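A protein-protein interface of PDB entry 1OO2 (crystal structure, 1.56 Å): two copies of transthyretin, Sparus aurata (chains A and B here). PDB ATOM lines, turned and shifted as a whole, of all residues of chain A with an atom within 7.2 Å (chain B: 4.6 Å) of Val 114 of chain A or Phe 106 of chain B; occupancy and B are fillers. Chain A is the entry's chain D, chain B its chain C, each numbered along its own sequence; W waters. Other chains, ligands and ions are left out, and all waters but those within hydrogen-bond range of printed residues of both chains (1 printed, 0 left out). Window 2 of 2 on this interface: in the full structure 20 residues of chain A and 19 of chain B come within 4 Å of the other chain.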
ATOM      1  N   PHE A  87      -3.838 -15.398 -17.754  1.00  0.00           N
ATOM      2  CA  PHE A  87      -3.247 -16.014 -16.580  1.00  0.00           C
ATOM      3  C   PHE A  87      -1.950 -16.759 -16.878  1.00  0.00           C
ATOM      4  O   PHE A  87      -1.764 -17.301 -17.972  1.00  0.00           O
ATOM      5  CB  PHE A  87      -4.258 -16.984 -15.941  1.00  0.00           C
ATOM      6  CG  PHE A  87      -4.602 -18.193 -16.789  1.00  0.00           C
ATOM      7  CD1 PHE A  87      -5.551 -18.060 -17.786  1.00  0.00           C
ATOM      8  CD2 PHE A  87      -3.984 -19.417 -16.588  1.00  0.00           C
ATOM      9  CE1 PHE A  87      -5.909 -19.121 -18.601  1.00  0.00           C
ATOM     10  CE2 PHE A  87      -4.347 -20.489 -17.393  1.00  0.00           C
ATOM     11  CZ  PHE A  87      -5.297 -20.332 -18.376  1.00  0.00           C
ATOM     12  N   HIS A  90       1.185 -23.019 -14.787  1.00  0.00           N
ATOM     13  CA  HIS A  90       2.277 -23.944 -14.506  1.00  0.00           C
ATOM     14  C   HIS A  90       1.727 -25.355 -14.368  1.00  0.00           C
ATOM     15  O   HIS A  90       1.507 -25.790 -13.232  1.00  0.00           O
ATOM     16  CB  HIS A  90       2.968 -23.534 -13.203  1.00  0.00           C
ATOM     17  CG  HIS A  90       3.438 -22.113 -13.259  1.00  0.00           C
ATOM     18  ND1 HIS A  90       4.589 -21.737 -13.912  1.00  0.00           N
ATOM     19  CD2 HIS A  90       2.891 -20.973 -12.772  1.00  0.00           C
ATOM     20  CE1 HIS A  90       4.748 -20.427 -13.811  1.00  0.00           C
ATOM     21  NE2 HIS A  90       3.731 -19.939 -13.118  1.00  0.00           N
ATOM     22  N   GLY A  95      -1.118 -30.020 -12.773  1.00  0.00           N
ATOM     23  CA  GLY A  95      -1.937 -28.912 -12.270  1.00  0.00           C
ATOM     24  C   GLY A  95      -2.959 -28.572 -13.349  1.00  0.00           C
ATOM     25  O   GLY A  95      -2.536 -28.190 -14.439  1.00  0.00           O
ATOM     26  N   HIS A  96      -4.237 -28.754 -13.050  1.00  0.00           N
ATOM     27  CA  HIS A  96      -5.318 -28.539 -14.000  1.00  0.00           C
ATOM     28  C   HIS A  96      -6.023 -27.215 -13.691  1.00  0.00           C
ATOM     29  O   HIS A  96      -6.040 -26.821 -12.530  1.00  0.00           O
ATOM     30  CB  HIS A  96      -6.333 -29.681 -13.931  1.00  0.00           C
ATOM     31  CG  HIS A  96      -5.712 -31.043 -13.993  1.00  0.00           C
ATOM     32  ND1 HIS A  96      -5.227 -31.679 -12.871  1.00  0.00           N
ATOM     33  CD2 HIS A  96      -5.499 -31.890 -15.021  1.00  0.00           C
ATOM     34  CE1 HIS A  96      -4.740 -32.861 -13.207  1.00  0.00           C
ATOM     35  NE2 HIS A  96      -4.896 -33.011 -14.509  1.00  0.00           N
ATOM     36  N   TYR A  97      -6.507 -26.582 -14.741  1.00  0.00           N
ATOM     37  CA  TYR A  97      -7.111 -25.256 -14.720  1.00  0.00           C
ATOM     38  C   TYR A  97      -8.546 -25.310 -15.236  1.00  0.00           C
ATOM     39  O   TYR A  97      -8.755 -25.816 -16.340  1.00  0.00           O
ATOM     40  CB  TYR A  97      -6.288 -24.299 -15.606  1.00  0.00           C
ATOM     41  CG  TYR A  97      -4.928 -24.030 -14.980  1.00  0.00           C
ATOM     42  CD1 TYR A  97      -3.879 -24.917 -15.187  1.00  0.00           C
ATOM     43  CD2 TYR A  97      -4.699 -22.918 -14.174  1.00  0.00           C
ATOM     44  CE1 TYR A  97      -2.641 -24.688 -14.619  1.00  0.00           C
ATOM     45  CE2 TYR A  97      -3.459 -22.695 -13.609  1.00  0.00           C
ATOM     46  CZ  TYR A  97      -2.429 -23.583 -13.835  1.00  0.00           C
ATOM     47  OH  TYR A  97      -1.200 -23.342 -13.253  1.00  0.00           O
ATOM     48  N   THR A  98      -9.502 -24.823 -14.451  1.00  0.00           N
ATOM     49  CA  THR A  98     -10.872 -24.641 -14.910  1.00  0.00           C
ATOM     50  C   THR A  98     -11.237 -23.162 -14.808  1.00  0.00           C
ATOM     51  O   THR A  98     -11.157 -22.562 -13.732  1.00  0.00           O
ATOM     52  CB  THR A  98     -11.875 -25.453 -14.070  1.00  0.00           C
ATOM     53  OG1 THR A  98     -11.524 -26.841 -14.095  1.00  0.00           O
ATOM     54  CG2 THR A  98     -13.277 -25.344 -14.668  1.00  0.00           C
ATOM     55  N   LEU A  99     -11.630 -22.575 -15.929  1.00  0.00           N
ATOM     56  CA  LEU A  99     -12.117 -21.199 -15.942  1.00  0.00           C
ATOM     57  C   LEU A  99     -13.645 -21.209 -15.975  1.00  0.00           C
ATOM     58  O   LEU A  99     -14.243 -21.678 -16.951  1.00  0.00           O
ATOM     59  CB  LEU A  99     -11.621 -20.444 -17.176  1.00  0.00           C
ATOM     60  CG  LEU A  99     -10.127 -20.587 -17.502  1.00  0.00           C
ATOM     61  CD1 LEU A  99      -9.828 -19.839 -18.801  1.00  0.00           C
ATOM     62  CD2 LEU A  99      -9.270 -20.090 -16.344  1.00  0.00           C
ATOM     63  N   THR A 110     -16.038 -14.059 -13.587  1.00  0.00           N
ATOM     64  CA  THR A 110     -15.175 -15.184 -13.951  1.00  0.00           C
ATOM     65  C   THR A 110     -14.292 -15.571 -12.773  1.00  0.00           C
ATOM     66  O   THR A 110     -13.874 -14.719 -11.993  1.00  0.00           O
ATOM     67  CB  THR A 110     -14.332 -14.898 -15.197  1.00  0.00           C
ATOM     68  OG1 THR A 110     -13.645 -16.109 -15.550  1.00  0.00           O
ATOM     69  CG2 THR A 110     -13.282 -13.824 -14.987  1.00  0.00           C
ATOM     70  N   THR A 111     -14.141 -16.887 -12.601  1.00  0.00           N
ATOM     71  CA  THR A 111     -13.379 -17.438 -11.479  1.00  0.00           C
ATOM     72  C   THR A 111     -12.471 -18.537 -12.003  1.00  0.00           C
ATOM     73  O   THR A 111     -12.726 -19.079 -13.085  1.00  0.00           O
ATOM     74  CB  THR A 111     -14.259 -17.976 -10.337  1.00  0.00           C
ATOM     75  OG1 THR A 111     -14.675 -19.331 -10.561  1.00  0.00           O
ATOM     76  CG2 THR A 111     -15.556 -17.192 -10.214  1.00  0.00           C
ATOM     77  N   ALA A 112     -11.415 -18.842 -11.253  1.00  0.00           N
ATOM     78  CA  ALA A 112     -10.631 -20.018 -11.632  1.00  0.00           C
ATOM     79  C   ALA A 112     -10.634 -21.052 -10.508  1.00  0.00           C
ATOM     80  O   ALA A 112     -10.692 -20.707  -9.335  1.00  0.00           O
ATOM     81  CB  ALA A 112      -9.208 -19.636 -12.004  1.00  0.00           C
ATOM     82  N   VAL A 113     -10.587 -22.317 -10.903  1.00  0.00           N
ATOM     83  CA  VAL A 113     -10.356 -23.450 -10.003  1.00  0.00           C
ATOM     84  C   VAL A 113      -9.089 -24.163 -10.457  1.00  0.00           C
ATOM     85  O   VAL A 113      -9.010 -24.613 -11.603  1.00  0.00           O
ATOM     86  CB  VAL A 113     -11.563 -24.390 -10.002  1.00  0.00           C
ATOM     87  CG1 VAL A 113     -11.341 -25.636  -9.162  1.00  0.00           C
ATOM     88  CG2 VAL A 113     -12.767 -23.614  -9.453  1.00  0.00           C
ATOM     89  N   VAL A 114      -8.093 -24.200  -9.584  1.00  0.00           N
ATOM     90  CA  VAL A 114      -6.807 -24.787  -9.949  1.00  0.00           C
ATOM     91  C   VAL A 114      -6.573 -25.992  -9.049  1.00  0.00           C
ATOM     92  O   VAL A 114      -6.653 -25.851  -7.825  1.00  0.00           O
ATOM     93  CB  VAL A 114      -5.667 -23.774  -9.752  1.00  0.00           C
ATOM     94  CG1 VAL A 114      -4.362 -24.386 -10.247  1.00  0.00           C
ATOM     95  CG2 VAL A 114      -5.972 -22.486 -10.505  1.00  0.00           C
ATOM     96  N   SER A 115      -6.305 -27.132  -9.674  1.00  0.00           N
ATOM     97  CA  SER A 115      -6.151 -28.370  -8.921  1.00  0.00           C
ATOM     98  C   SER A 115      -4.773 -28.467  -8.279  1.00  0.00           C
ATOM     99  O   SER A 115      -3.880 -27.672  -8.583  1.00  0.00           O
ATOM    100  CB  SER A 115      -6.366 -29.560  -9.876  1.00  0.00           C
ATOM    101  OG  SER A 115      -5.157 -29.761 -10.598  1.00  0.00           O
ATOM    102  N   SER A 116      -4.620 -29.444  -7.390  1.00  0.00           N
ATOM    103  CA  SER A 116      -3.359 -29.713  -6.711  1.00  0.00           C
ATOM    104  C   SER A 116      -3.000 -31.195  -6.823  1.00  0.00           C
ATOM    105  O   SER A 116      -3.580 -31.191  -5.650  1.00  0.00           O
ATOM    106  CB  SER A 116      -3.431 -29.307  -5.237  1.00  0.00           C
ATOM    107  OG  SER A 116      -2.198 -28.781  -4.778  1.00  0.00           O
ATOM    108  N   THR B  77      -1.504 -13.585  -3.453  1.00  0.00           N
ATOM    109  CA  THR B  77      -1.127 -13.987  -4.807  1.00  0.00           C
ATOM    110  C   THR B  77      -2.396 -14.179  -5.651  1.00  0.00           C
ATOM    111  O   THR B  77      -3.323 -14.911  -5.305  1.00  0.00           O
ATOM    112  CB  THR B  77      -0.292 -15.272  -4.881  1.00  0.00           C
ATOM    113  OG1 THR B  77       0.870 -15.170  -4.045  1.00  0.00           O
ATOM    114  CG2 THR B  77       0.241 -15.487  -6.295  1.00  0.00           C
ATOM    115  N   PHE B  79      -4.671 -14.896  -9.284  1.00  0.00           N
ATOM    116  CA  PHE B  79      -4.669 -15.743 -10.466  1.00  0.00           C
ATOM    117  C   PHE B  79      -4.420 -14.969 -11.760  1.00  0.00           C
ATOM    118  O   PHE B  79      -3.598 -15.408 -12.563  1.00  0.00           O
ATOM    119  CB  PHE B  79      -6.018 -16.466 -10.557  1.00  0.00           C
ATOM    120  CG  PHE B  79      -6.173 -17.354 -11.780  1.00  0.00           C
ATOM    121  CD1 PHE B  79      -5.541 -18.591 -11.799  1.00  0.00           C
ATOM    122  CD2 PHE B  79      -6.931 -16.975 -12.864  1.00  0.00           C
ATOM    123  CE1 PHE B  79      -5.659 -19.416 -12.907  1.00  0.00           C
ATOM    124  CE2 PHE B  79      -7.058 -17.783 -13.990  1.00  0.00           C
ATOM    125  CZ  PHE B  79      -6.423 -19.011 -13.983  1.00  0.00           C
ATOM    126  N   HIS B  80      -5.176 -13.911 -12.002  1.00  0.00           N
ATOM    127  CA  HIS B  80      -5.202 -13.258 -13.299  1.00  0.00           C
ATOM    128  C   HIS B  80      -4.018 -12.301 -13.473  1.00  0.00           C
ATOM    129  O   HIS B  80      -3.580 -11.655 -12.526  1.00  0.00           O
ATOM    130  CB  HIS B  80      -6.496 -12.478 -13.535  1.00  0.00           C
ATOM    131  CG  HIS B  80      -7.745 -13.290 -13.391  1.00  0.00           C
ATOM    132  ND1 HIS B  80      -8.408 -13.463 -12.192  1.00  0.00           N
ATOM    133  CD2 HIS B  80      -8.416 -14.002 -14.334  1.00  0.00           C
ATOM    134  CE1 HIS B  80      -9.461 -14.239 -12.405  1.00  0.00           C
ATOM    135  NE2 HIS B  80      -9.486 -14.576 -13.684  1.00  0.00           N
ATOM    136  N   SER B 104     -11.618 -10.365  -6.233  1.00  0.00           N
ATOM    137  CA  SER B 104     -11.105 -11.356  -5.291  1.00  0.00           C
ATOM    138  C   SER B 104      -9.827 -11.927  -5.898  1.00  0.00           C
ATOM    139  O   SER B 104      -9.653 -11.796  -7.119  1.00  0.00           O
ATOM    140  CB  SER B 104     -12.088 -12.501  -5.050  1.00  0.00           C
ATOM    141  OG  SER B 104     -13.357 -12.003  -4.666  1.00  0.00           O
ATOM    142  N   PRO B 105      -8.940 -12.517  -5.121  1.00  0.00           N
ATOM    143  CA  PRO B 105      -7.702 -13.036  -5.723  1.00  0.00           C
ATOM    144  C   PRO B 105      -7.912 -13.958  -6.908  1.00  0.00           C
ATOM    145  O   PRO B 105      -7.126 -13.852  -7.859  1.00  0.00           O
ATOM    146  CB  PRO B 105      -7.062 -13.770  -4.528  1.00  0.00           C
ATOM    147  CG  PRO B 105      -7.479 -12.918  -3.361  1.00  0.00           C
ATOM    148  CD  PRO B 105      -8.947 -12.629  -3.645  1.00  0.00           C
ATOM    149  N   PHE B 106      -8.913 -14.842  -6.904  1.00  0.00           N
ATOM    150  CA  PHE B 106      -9.106 -15.786  -8.006  1.00  0.00           C
ATOM    151  C   PHE B 106     -10.369 -15.512  -8.825  1.00  0.00           C
ATOM    152  O   PHE B 106     -10.813 -16.342  -9.637  1.00  0.00           O
ATOM    153  CB  PHE B 106      -9.122 -17.231  -7.470  1.00  0.00           C
ATOM    154  CG  PHE B 106      -7.729 -17.850  -7.354  1.00  0.00           C
ATOM    155  CD1 PHE B 106      -7.326 -18.854  -8.224  1.00  0.00           C
ATOM    156  CD2 PHE B 106      -6.835 -17.424  -6.387  1.00  0.00           C
ATOM    157  CE1 PHE B 106      -6.078 -19.448  -8.122  1.00  0.00           C
ATOM    158  CE2 PHE B 106      -5.593 -18.027  -6.255  1.00  0.00           C
ATOM    159  CZ  PHE B 106      -5.215 -19.032  -7.126  1.00  0.00           C
ATOM    160  N   SER B 107     -10.967 -14.331  -8.653  1.00  0.00           N
ATOM    161  CA  SER B 107     -12.224 -14.050  -9.354  1.00  0.00           C
ATOM    162  C   SER B 107     -12.427 -12.562  -9.575  1.00  0.00           C
ATOM    163  O   SER B 107     -11.989 -11.716  -8.792  1.00  0.00           O
ATOM    164  CB  SER B 107     -13.409 -14.564  -8.506  1.00  0.00           C
ATOM    165  OG  SER B 107     -14.636 -14.486  -9.222  1.00  0.00           O
HETATM  166  O   HOH W   1     -11.097 -16.896 -14.656  1.00  0.00           O
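Water W1 lies within hydrogen-bond range of OG1 of Thr 110 of chain A (2.8 Å), NE2 of His 80 of chain B (3.0 Å) and O of Thr 111 of chain A (3.1 Å).
Of the printed residues of chain B, Phe 87 of chain A touches Phe 79 (3.4 Å).
Of the printed residues of chain B, Ala 112 of chain A touches Phe 79 (3.5 Å) and Phe 106 (3.0 Å).
Of the printed residues of chain B, Val 114 of chain A touches Phe 79 (3.9 Å) and Phe 106 (3.9 Å).
Ser 104 of chain B touches none of the printed residues of chain A.
Phe 106 of chain B touches just these residues of chain A: Thr 111, Ala 112 and Val 114.
The nearest printed residue of chain A that does not touch Phe 79 of chain B is Thr 111 of chain A (5.8 Å).
N of Phe 79 of chain B lies within hydrogen-bond range of O of Pro 105 of chain B.
N of His 90 of chain A is in hydrogen-bond range of OH of Tyr 97 of chain A (2.9 Å).
No position is printed for both chains.
Of the 10 pairs that touch across the chains among the printed residues, none has its exchanged pair printed and touching as well.
Of the 7 printed residues of chain B, 3 touch a printed residue of chain A.
Hydrophobic or aromatic side chains of chain B within 4 Å of the printed part of chain A: Phe 79 and Phe 106.
OG of Ser 107 of chain B is in hydrogen-bond range of O of Thr 110 of chain A (2.9 Å).
The backbone carbonyl oxygen of Phe 106 of chain B lies within hydrogen-bond range of the backbone NH of Ala 112 of chain A.
CZ of Phe 79 of chain B touches CG of Phe 87 of chain A, 3.4 Å away.
Tyr 97 of chain A touches Phe 79 of chain B (CD2 to CE1, 3.8 Å).
Leu 99 of chain A touches Phe 79 of chain B.
CA of Thr 111 of chain A touches O of Phe 106 of chain B, at 3.3 Å.
OG of Ser 107 of chain B touches CG2 of Thr 111 of chain A, at 3.0 Å.
CE2 of Phe 79 of chain B touches CB of Ala 112 of chain A (3.5 Å).
Phe 79 of chain B touches Val 114 of chain A (CE1 to CG2, 3.9 Å).
Val 114 of chain A touches Phe 106 of chain B (CG2 to CE1, 3.9 Å).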
